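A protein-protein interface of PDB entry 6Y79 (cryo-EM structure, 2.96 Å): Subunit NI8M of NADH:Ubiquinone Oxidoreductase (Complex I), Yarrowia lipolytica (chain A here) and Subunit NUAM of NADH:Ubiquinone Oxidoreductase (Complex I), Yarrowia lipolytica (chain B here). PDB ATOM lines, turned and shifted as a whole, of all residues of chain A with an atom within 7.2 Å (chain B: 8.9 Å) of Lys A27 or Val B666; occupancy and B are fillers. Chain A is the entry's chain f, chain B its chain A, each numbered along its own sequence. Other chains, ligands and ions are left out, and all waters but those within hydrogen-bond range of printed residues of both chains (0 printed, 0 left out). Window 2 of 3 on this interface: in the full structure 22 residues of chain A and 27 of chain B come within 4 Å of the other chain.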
ATOM      1  N   LEU A  12      22.601 -22.610  27.489  1.00  0.00           N
ATOM      2  CA  LEU A  12      22.360 -21.288  28.040  1.00  0.00           C
ATOM      3  C   LEU A  12      20.894 -20.930  27.861  1.00  0.00           C
ATOM      4  O   LEU A  12      20.168 -21.543  27.071  1.00  0.00           O
ATOM      5  CB  LEU A  12      23.190 -20.193  27.342  1.00  0.00           C
ATOM      6  CG  LEU A  12      24.682 -20.129  27.393  1.00  0.00           C
ATOM      7  CD1 LEU A  12      25.300 -21.001  26.321  1.00  0.00           C
ATOM      8  CD2 LEU A  12      25.139 -18.693  27.194  1.00  0.00           C
ATOM      9  N   CYS A  13      20.474 -19.894  28.571  1.00  0.00           N
ATOM     10  CA  CYS A  13      19.331 -19.116  28.136  1.00  0.00           C
ATOM     11  C   CYS A  13      19.825 -17.752  27.683  1.00  0.00           C
ATOM     12  O   CYS A  13      20.734 -17.174  28.287  1.00  0.00           O
ATOM     13  CB  CYS A  13      18.279 -18.996  29.233  1.00  0.00           C
ATOM     14  SG  CYS A  13      18.772 -18.085  30.649  1.00  0.00           S
ATOM     15  N   GLN A  14      19.244 -17.259  26.590  1.00  0.00           N
ATOM     16  CA  GLN A  14      19.828 -16.126  25.879  1.00  0.00           C
ATOM     17  C   GLN A  14      19.704 -14.820  26.646  1.00  0.00           C
ATOM     18  O   GLN A  14      20.633 -14.005  26.620  1.00  0.00           O
ATOM     19  CB  GLN A  14      19.164 -15.957  24.524  1.00  0.00           C
ATOM     20  CG  GLN A  14      19.439 -17.053  23.562  1.00  0.00           C
ATOM     21  CD  GLN A  14      18.748 -16.796  22.268  1.00  0.00           C
ATOM     22  OE1 GLN A  14      17.943 -15.870  22.153  1.00  0.00           O
ATOM     23  NE2 GLN A  14      19.070 -17.593  21.267  1.00  0.00           N
ATOM     24  N   ASN A  15      18.566 -14.584  27.290  1.00  0.00           N
ATOM     25  CA  ASN A  15      18.376 -13.339  28.013  1.00  0.00           C
ATOM     26  C   ASN A  15      18.890 -13.467  29.440  1.00  0.00           C
ATOM     27  O   ASN A  15      18.862 -14.540  30.043  1.00  0.00           O
ATOM     28  CB  ASN A  15      16.904 -12.916  27.955  1.00  0.00           C
ATOM     29  CG  ASN A  15      16.623 -12.064  26.738  1.00  0.00           C
ATOM     30  OD1 ASN A  15      17.565 -11.540  26.144  1.00  0.00           O
ATOM     31  ND2 ASN A  15      15.357 -11.890  26.377  1.00  0.00           N
ATOM     32  N   PRO A  21      27.416 -14.911  33.482  1.00  0.00           N
ATOM     33  CA  PRO A  21      28.825 -15.296  33.699  1.00  0.00           C
ATOM     34  C   PRO A  21      29.275 -16.431  32.803  1.00  0.00           C
ATOM     35  O   PRO A  21      30.387 -16.381  32.256  1.00  0.00           O
ATOM     36  CB  PRO A  21      28.857 -15.696  35.182  1.00  0.00           C
ATOM     37  CG  PRO A  21      27.453 -16.035  35.510  1.00  0.00           C
ATOM     38  CD  PRO A  21      26.682 -15.018  34.764  1.00  0.00           C
ATOM     39  N   LEU A  22      28.410 -17.428  32.586  1.00  0.00           N
ATOM     40  CA  LEU A  22      28.687 -18.458  31.587  1.00  0.00           C
ATOM     41  C   LEU A  22      28.821 -17.856  30.187  1.00  0.00           C
ATOM     42  O   LEU A  22      29.649 -18.313  29.402  1.00  0.00           O
ATOM     43  CB  LEU A  22      27.593 -19.541  31.615  1.00  0.00           C
ATOM     44  CG  LEU A  22      27.906 -20.929  31.003  1.00  0.00           C
ATOM     45  CD1 LEU A  22      27.064 -21.987  31.658  1.00  0.00           C
ATOM     46  CD2 LEU A  22      27.674 -20.996  29.514  1.00  0.00           C
ATOM     47  N   ARG A  23      28.053 -16.805  29.882  1.00  0.00           N
ATOM     48  CA  ARG A  23      28.036 -16.261  28.530  1.00  0.00           C
ATOM     49  C   ARG A  23      29.331 -15.514  28.219  1.00  0.00           C
ATOM     50  O   ARG A  23      29.852 -15.575  27.102  1.00  0.00           O
ATOM     51  CB  ARG A  23      26.839 -15.356  28.356  1.00  0.00           C
ATOM     52  CG  ARG A  23      26.654 -14.811  26.949  1.00  0.00           C
ATOM     53  CD  ARG A  23      25.339 -14.078  26.803  1.00  0.00           C
ATOM     54  NE  ARG A  23      24.239 -14.839  27.377  1.00  0.00           N
ATOM     55  CZ  ARG A  23      23.518 -14.436  28.417  1.00  0.00           C
ATOM     56  NH1 ARG A  23      22.538 -15.195  28.882  1.00  0.00           N
ATOM     57  NH2 ARG A  23      23.798 -13.284  29.005  1.00  0.00           N
ATOM     58  N   GLN A  24      29.885 -14.791  29.178  1.00  0.00           N
ATOM     59  CA  GLN A  24      31.207 -14.212  28.929  1.00  0.00           C
ATOM     60  C   GLN A  24      32.326 -15.244  29.053  1.00  0.00           C
ATOM     61  O   GLN A  24      33.375 -15.067  28.415  1.00  0.00           O
ATOM     62  CB  GLN A  24      31.440 -13.017  29.855  1.00  0.00           C
ATOM     63  CG  GLN A  24      31.229 -13.203  31.329  1.00  0.00           C
ATOM     64  CD  GLN A  24      31.555 -11.916  32.037  1.00  0.00           C
ATOM     65  OE1 GLN A  24      31.793 -10.900  31.379  1.00  0.00           O
ATOM     66  NE2 GLN A  24      31.690 -11.968  33.353  1.00  0.00           N
ATOM     67  N   PHE A  25      32.090 -16.360  29.779  1.00  0.00           N
ATOM     68  CA  PHE A  25      33.016 -17.490  29.699  1.00  0.00           C
ATOM     69  C   PHE A  25      33.028 -18.094  28.300  1.00  0.00           C
ATOM     70  O   PHE A  25      34.090 -18.529  27.827  1.00  0.00           O
ATOM     71  CB  PHE A  25      32.673 -18.573  30.717  1.00  0.00           C
ATOM     72  CG  PHE A  25      33.688 -19.713  30.752  1.00  0.00           C
ATOM     73  CD1 PHE A  25      34.915 -19.549  31.382  1.00  0.00           C
ATOM     74  CD2 PHE A  25      33.422 -20.931  30.132  1.00  0.00           C
ATOM     75  CE1 PHE A  25      35.854 -20.576  31.412  1.00  0.00           C
ATOM     76  CE2 PHE A  25      34.352 -21.963  30.155  1.00  0.00           C
ATOM     77  CZ  PHE A  25      35.574 -21.783  30.795  1.00  0.00           C
ATOM     78  N   VAL A  26      31.861 -18.147  27.636  1.00  0.00           N
ATOM     79  CA  VAL A  26      31.842 -18.436  26.197  1.00  0.00           C
ATOM     80  C   VAL A  26      32.742 -17.467  25.470  1.00  0.00           C
ATOM     81  O   VAL A  26      33.845 -17.835  25.057  1.00  0.00           O
ATOM     82  CB  VAL A  26      30.416 -18.379  25.607  1.00  0.00           C
ATOM     83  CG1 VAL A  26      30.392 -18.656  24.083  1.00  0.00           C
ATOM     84  CG2 VAL A  26      29.391 -19.342  26.344  1.00  0.00           C
ATOM     85  N   LYS A  27      32.365 -16.193  25.473  1.00  0.00           N
ATOM     86  CA  LYS A  27      32.935 -15.209  24.555  1.00  0.00           C
ATOM     87  C   LYS A  27      34.425 -14.969  24.745  1.00  0.00           C
ATOM     88  O   LYS A  27      35.066 -14.462  23.821  1.00  0.00           O
ATOM     89  CB  LYS A  27      32.169 -13.873  24.660  1.00  0.00           C
ATOM     90  CG  LYS A  27      30.722 -14.028  24.299  1.00  0.00           C
ATOM     91  CD  LYS A  27      30.019 -12.694  24.376  1.00  0.00           C
ATOM     92  CE  LYS A  27      28.561 -12.795  23.977  1.00  0.00           C
ATOM     93  NZ  LYS A  27      27.906 -11.463  24.033  1.00  0.00           N
ATOM     94  N   ASN A  28      35.013 -15.397  25.861  1.00  0.00           N
ATOM     95  CA  ASN A  28      36.468 -15.353  25.907  1.00  0.00           C
ATOM     96  C   ASN A  28      37.177 -16.716  25.905  1.00  0.00           C
ATOM     97  O   ASN A  28      38.358 -16.758  25.536  1.00  0.00           O
ATOM     98  CB  ASN A  28      36.950 -14.500  27.091  1.00  0.00           C
ATOM     99  CG  ASN A  28      36.743 -15.154  28.441  1.00  0.00           C
ATOM    100  OD1 ASN A  28      35.945 -16.071  28.608  1.00  0.00           O
ATOM    101  ND2 ASN A  28      37.507 -14.695  29.416  1.00  0.00           N
ATOM    102  N   GLN A  29      36.538 -17.844  26.250  1.00  0.00           N
ATOM    103  CA  GLN A  29      37.309 -19.076  26.369  1.00  0.00           C
ATOM    104  C   GLN A  29      36.982 -20.145  25.331  1.00  0.00           C
ATOM    105  O   GLN A  29      37.489 -21.279  25.482  1.00  0.00           O
ATOM    106  CB  GLN A  29      37.163 -19.666  27.780  1.00  0.00           C
ATOM    107  CG  GLN A  29      37.752 -18.796  28.893  1.00  0.00           C
ATOM    108  CD  GLN A  29      39.244 -18.534  28.734  1.00  0.00           C
ATOM    109  OE1 GLN A  29      40.024 -19.440  28.440  1.00  0.00           O
ATOM    110  NE2 GLN A  29      39.644 -17.280  28.925  1.00  0.00           N
ATOM    111  N   ILE A  30      36.185 -19.829  24.289  1.00  0.00           N
ATOM    112  CA  ILE A  30      35.976 -20.811  23.208  1.00  0.00           C
ATOM    113  C   ILE A  30      37.303 -21.229  22.558  1.00  0.00           C
ATOM    114  O   ILE A  30      37.640 -22.427  22.493  1.00  0.00           O
ATOM    115  CB  ILE A  30      35.018 -20.266  22.140  1.00  0.00           C
ATOM    116  CG1 ILE A  30      33.668 -19.924  22.724  1.00  0.00           C
ATOM    117  CG2 ILE A  30      34.843 -21.317  21.062  1.00  0.00           C
ATOM    118  CD1 ILE A  30      32.970 -21.093  23.327  1.00  0.00           C
ATOM    119  N   GLY A  31      38.068 -20.246  22.071  1.00  0.00           N
ATOM    120  CA  GLY A  31      39.288 -20.541  21.337  1.00  0.00           C
ATOM    121  C   GLY A  31      40.387 -21.135  22.191  1.00  0.00           C
ATOM    122  O   GLY A  31      41.259 -21.845  21.680  1.00  0.00           O
ATOM    123  N   GLU A  46      21.273 -22.821  22.882  1.00  0.00           N
ATOM    124  CA  GLU A  46      20.638 -21.658  23.487  1.00  0.00           C
ATOM    125  C   GLU A  46      19.133 -21.741  23.306  1.00  0.00           C
ATOM    126  O   GLU A  46      18.652 -21.985  22.193  1.00  0.00           O
ATOM    127  CB  GLU A  46      21.150 -20.358  22.852  1.00  0.00           C
ATOM    128  CG  GLU A  46      22.577 -19.992  23.152  1.00  0.00           C
ATOM    129  CD  GLU A  46      23.565 -20.662  22.179  1.00  0.00           C
ATOM    130  OE1 GLU A  46      23.114 -21.146  21.139  1.00  0.00           O
ATOM    131  OE2 GLU A  46      24.745 -20.770  22.536  1.00  0.00           O
ATOM    132  N   PHE B 391      28.341 -23.248  17.692  1.00  0.00           N
ATOM    133  CA  PHE B 391      27.686 -21.970  17.413  1.00  0.00           C
ATOM    134  C   PHE B 391      26.696 -22.051  16.265  1.00  0.00           C
ATOM    135  O   PHE B 391      27.077 -21.688  15.151  1.00  0.00           O
ATOM    136  CB  PHE B 391      28.709 -20.872  17.118  1.00  0.00           C
ATOM    137  CG  PHE B 391      29.561 -20.507  18.286  1.00  0.00           C
ATOM    138  CD1 PHE B 391      29.088 -19.645  19.262  1.00  0.00           C
ATOM    139  CD2 PHE B 391      30.842 -21.019  18.404  1.00  0.00           C
ATOM    140  CE1 PHE B 391      29.876 -19.304  20.340  1.00  0.00           C
ATOM    141  CE2 PHE B 391      31.636 -20.683  19.477  1.00  0.00           C
ATOM    142  CZ  PHE B 391      31.152 -19.824  20.447  1.00  0.00           C
ATOM    143  N   SER B 393      24.485 -20.646  14.635  1.00  0.00           N
ATOM    144  CA  SER B 393      24.470 -19.585  13.633  1.00  0.00           C
ATOM    145  C   SER B 393      25.513 -19.715  12.521  1.00  0.00           C
ATOM    146  O   SER B 393      25.505 -18.929  11.572  1.00  0.00           O
ATOM    147  CB  SER B 393      24.632 -18.226  14.323  1.00  0.00           C
ATOM    148  OG  SER B 393      25.915 -18.092  14.904  1.00  0.00           O
ATOM    149  N   LEU B 512      26.555  -7.387   9.809  1.00  0.00           N
ATOM    150  CA  LEU B 512      26.485  -8.080  11.093  1.00  0.00           C
ATOM    151  C   LEU B 512      26.501  -7.045  12.210  1.00  0.00           C
ATOM    152  O   LEU B 512      27.546  -6.447  12.488  1.00  0.00           O
ATOM    153  CB  LEU B 512      27.643  -9.066  11.242  1.00  0.00           C
ATOM    154  CG  LEU B 512      27.702  -9.882  12.534  1.00  0.00           C
ATOM    155  CD1 LEU B 512      26.454 -10.722  12.705  1.00  0.00           C
ATOM    156  CD2 LEU B 512      28.955 -10.749  12.544  1.00  0.00           C
ATOM    157  N   ASN B 513      25.355  -6.842  12.850  1.00  0.00           N
ATOM    158  CA  ASN B 513      25.231  -5.916  13.976  1.00  0.00           C
ATOM    159  C   ASN B 513      24.333  -6.575  15.021  1.00  0.00           C
ATOM    160  O   ASN B 513      24.165  -7.799  15.037  1.00  0.00           O
ATOM    161  CB  ASN B 513      24.769  -4.517  13.512  1.00  0.00           C
ATOM    162  CG  ASN B 513      23.394  -4.503  12.840  1.00  0.00           C
ATOM    163  OD1 ASN B 513      22.679  -5.503  12.781  1.00  0.00           O
ATOM    164  ND2 ASN B 513      23.023  -3.337  12.328  1.00  0.00           N
ATOM    165  N   GLU B 514      23.783  -5.767  15.931  1.00  0.00           N
ATOM    166  CA  GLU B 514      22.978  -6.303  17.025  1.00  0.00           C
ATOM    167  C   GLU B 514      21.646  -6.858  16.523  1.00  0.00           C
ATOM    168  O   GLU B 514      21.382  -8.060  16.640  1.00  0.00           O
ATOM    169  CB  GLU B 514      22.747  -5.222  18.088  1.00  0.00           C
ATOM    170  CG  GLU B 514      24.010  -4.788  18.842  1.00  0.00           C
ATOM    171  CD  GLU B 514      23.772  -3.663  19.843  1.00  0.00           C
ATOM    172  OE1 GLU B 514      22.672  -3.075  19.835  1.00  0.00           O
ATOM    173  OE2 GLU B 514      24.685  -3.388  20.646  1.00  0.00           O
ATOM    174  N   ASN B 517      21.051 -10.278  11.695  1.00  0.00           N
ATOM    175  CA  ASN B 517      22.228 -11.013  11.251  1.00  0.00           C
ATOM    176  C   ASN B 517      22.104 -11.260   9.754  1.00  0.00           C
ATOM    177  O   ASN B 517      21.002 -11.483   9.246  1.00  0.00           O
ATOM    178  CB  ASN B 517      22.342 -12.335  12.032  1.00  0.00           C
ATOM    179  CG  ASN B 517      23.644 -13.091  11.782  1.00  0.00           C
ATOM    180  OD1 ASN B 517      24.465 -12.728  10.942  1.00  0.00           O
ATOM    181  ND2 ASN B 517      23.838 -14.156  12.549  1.00  0.00           N
ATOM    182  N   GLU B 663      14.450 -18.231  18.058  1.00  0.00           N
ATOM    183  CA  GLU B 663      15.311 -17.480  18.946  1.00  0.00           C
ATOM    184  C   GLU B 663      16.320 -16.662  18.145  1.00  0.00           C
ATOM    185  O   GLU B 663      16.656 -17.015  17.009  1.00  0.00           O
ATOM    186  CB  GLU B 663      16.046 -18.437  19.894  1.00  0.00           C
ATOM    187  CG  GLU B 663      17.105 -19.331  19.235  1.00  0.00           C
ATOM    188  CD  GLU B 663      16.546 -20.614  18.626  1.00  0.00           C
ATOM    189  OE1 GLU B 663      15.317 -20.719  18.432  1.00  0.00           O
ATOM    190  OE2 GLU B 663      17.350 -21.524  18.333  1.00  0.00           O
ATOM    191  N   PRO B 664      16.793 -15.543  18.676  1.00  0.00           N
ATOM    192  CA  PRO B 664      17.934 -14.849  18.074  1.00  0.00           C
ATOM    193  C   PRO B 664      19.240 -15.523  18.490  1.00  0.00           C
ATOM    194  O   PRO B 664      19.252 -16.567  19.135  1.00  0.00           O
ATOM    195  CB  PRO B 664      17.820 -13.431  18.636  1.00  0.00           C
ATOM    196  CG  PRO B 664      17.105 -13.602  19.927  1.00  0.00           C
ATOM    197  CD  PRO B 664      16.139 -14.730  19.716  1.00  0.00           C
ATOM    198  N   THR B 665      20.354 -14.921  18.082  1.00  0.00           N
ATOM    199  CA  THR B 665      21.679 -15.382  18.487  1.00  0.00           C
ATOM    200  C   THR B 665      22.455 -14.202  19.046  1.00  0.00           C
ATOM    201  O   THR B 665      22.682 -13.214  18.342  1.00  0.00           O
ATOM    202  CB  THR B 665      22.457 -16.013  17.325  1.00  0.00           C
ATOM    203  OG1 THR B 665      22.635 -15.047  16.281  1.00  0.00           O
ATOM    204  CG2 THR B 665      21.746 -17.244  16.775  1.00  0.00           C
ATOM    205  N   VAL B 666      22.860 -14.309  20.312  1.00  0.00           N
ATOM    206  CA  VAL B 666      23.768 -13.328  20.894  1.00  0.00           C
ATOM    207  C   VAL B 666      25.214 -13.600  20.473  1.00  0.00           C
ATOM    208  O   VAL B 666      26.072 -12.713  20.586  1.00  0.00           O
ATOM    209  CB  VAL B 666      23.539 -13.324  22.421  1.00  0.00           C
ATOM    210  CG1 VAL B 666      23.937 -14.654  23.041  1.00  0.00           C
ATOM    211  CG2 VAL B 666      24.210 -12.134  23.124  1.00  0.00           C
ATOM    212  N   PHE B 667      25.495 -14.777  19.910  1.00  0.00           N
ATOM    213  CA  PHE B 667      26.852 -15.200  19.578  1.00  0.00           C
ATOM    214  C   PHE B 667      27.205 -14.973  18.109  1.00  0.00           C
ATOM    215  O   PHE B 667      28.103 -15.643  17.579  1.00  0.00           O
ATOM    216  CB  PHE B 667      27.048 -16.674  19.931  1.00  0.00           C
ATOM    217  CG  PHE B 667      27.052 -16.957  21.407  1.00  0.00           C
ATOM    218  CD1 PHE B 667      27.239 -15.941  22.331  1.00  0.00           C
ATOM    219  CD2 PHE B 667      26.874 -18.251  21.870  1.00  0.00           C
ATOM    220  CE1 PHE B 667      27.237 -16.205  23.678  1.00  0.00           C
ATOM    221  CE2 PHE B 667      26.877 -18.523  23.225  1.00  0.00           C
ATOM    222  CZ  PHE B 667      27.058 -17.497  24.128  1.00  0.00           C
ATOM    223  N   GLY B 668      26.526 -14.032  17.445  1.00  0.00           N
ATOM    224  CA  GLY B 668      26.774 -13.803  16.031  1.00  0.00           C
ATOM    225  C   GLY B 668      28.137 -13.205  15.737  1.00  0.00           C
ATOM    226  O   GLY B 668      28.731 -13.497  14.695  1.00  0.00           O
ATOM    227  N   ASP B 669      28.651 -12.373  16.647  1.00  0.00           N
ATOM    228  CA  ASP B 669      29.989 -11.813  16.486  1.00  0.00           C
ATOM    229  C   ASP B 669      31.056 -12.884  16.682  1.00  0.00           C
ATOM    230  O   ASP B 669      31.997 -12.984  15.885  1.00  0.00           O
ATOM    231  CB  ASP B 669      30.181 -10.661  17.483  1.00  0.00           C
ATOM    232  CG  ASP B 669      31.420  -9.812  17.202  1.00  0.00           C
ATOM    233  OD1 ASP B 669      32.167 -10.082  16.239  1.00  0.00           O
ATOM    234  OD2 ASP B 669      31.643  -8.848  17.968  1.00  0.00           O
ATOM    235  N   VAL B 670      30.915 -13.701  17.731  1.00  0.00           N
ATOM    236  CA  VAL B 670      31.928 -14.696  18.074  1.00  0.00           C
ATOM    237  C   VAL B 670      31.959 -15.827  17.046  1.00  0.00           C
ATOM    238  O   VAL B 670      33.039 -16.345  16.717  1.00  0.00           O
ATOM    239  CB  VAL B 670      31.664 -15.208  19.505  1.00  0.00           C
ATOM    240  CG1 VAL B 670      32.653 -16.295  19.915  1.00  0.00           C
ATOM    241  CG2 VAL B 670      31.703 -14.052  20.495  1.00  0.00           C
ATOM    242  N   ALA B 671      30.795 -16.189  16.490  1.00  0.00           N
ATOM    243  CA  ALA B 671      30.707 -17.341  15.594  1.00  0.00           C
ATOM    244  C   ALA B 671      31.421 -17.098  14.268  1.00  0.00           C
ATOM    245  O   ALA B 671      32.049 -18.015  13.723  1.00  0.00           O
ATOM    246  CB  ALA B 671      29.242 -17.688  15.345  1.00  0.00           C
ATOM    247  N   GLN B 673      34.028 -15.099  13.745  1.00  0.00           N
ATOM    248  CA  GLN B 673      35.462 -15.189  14.010  1.00  0.00           C
ATOM    249  C   GLN B 673      35.905 -16.634  14.209  1.00  0.00           C
ATOM    250  O   GLN B 673      36.955 -17.045  13.692  1.00  0.00           O
ATOM    251  CB  GLN B 673      35.818 -14.351  15.239  1.00  0.00           C
ATOM    252  CG  GLN B 673      37.299 -14.313  15.553  1.00  0.00           C
ATOM    253  CD  GLN B 673      38.097 -13.602  14.477  1.00  0.00           C
ATOM    254  OE1 GLN B 673      37.678 -12.567  13.957  1.00  0.00           O
ATOM    255  NE2 GLN B 673      39.252 -14.159  14.132  1.00  0.00           N
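Val B666 touches just one residue of chain A: Lys A27.
Val A26 touches just these residues of chain B: Phe B391 and Phe B667.
Of the printed residues of chain B, Arg A23 touches Phe B667.
Of the printed residues of chain A, Pro B664 touches Gln A14.
Of the printed residues of chain B, Gln A14 touches Glu B663 and Pro B664.
Of the printed residues of chain A, Glu B663 touches Gln A14 (3.3 Å).
Of the printed residues of chain B, Glu A46 touches Phe B667 (3.2 Å).
The nearest printed residue of chain B that does not touch Glu A46 is Glu B663 (4.1 Å).
The backbone carbonyl oxygen of Cys A13 is in hydrogen-bond range of the guanidinium group of Arg A23 (2.7 Å).
The backbone carbonyl oxygen (O) of Gln A14 sits at hydrogen-bond distance from the guanidinium group (NH1) of Arg A23 (3.2 Å).
Of the 16 printed residues of chain B, 6 touch a printed residue of chain A.
Printed residues of chain B that touch a printed residue of chain A: Phe B391, Glu B663, Pro B664, Val B666, Phe B667 and Val B670.
Hydrophobic or aromatic side chains of chain B within 4 Å of the printed part of chain A: Phe B391, Pro B664, Val B666, Phe B667 and Val B670.
Hydrophobic or aromatic side chains of chain A within 4 Å of the printed part of chain B: Leu A12, Val A26 and Ile A30.
Among the printed residues, 11 pairs touch across the chains.
The backbone carbonyl oxygen of Pro B664 sits close to the side-chain amide oxygen of Gln A14.
Phe B667 touches Leu A12 (CZ to CD2, 3.8 Å).
CG of Glu B663 touches NE2 of Gln A14 (3.3 Å).
Arg A23 touches Phe B667.
Phe B391 touches Val A26.
Phe B667 touches Val A26.
CG2 of Val B666 touches NZ of Lys A27, 3.9 Å away.
Lys A27 touches Phe B667.
Lys A27 touches Val B670 (CG to CG2, 3.9 Å).
CG1 of Ile A30 touches CZ of Phe B391 (3.4 Å).
Phe B667 touches Glu A46.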
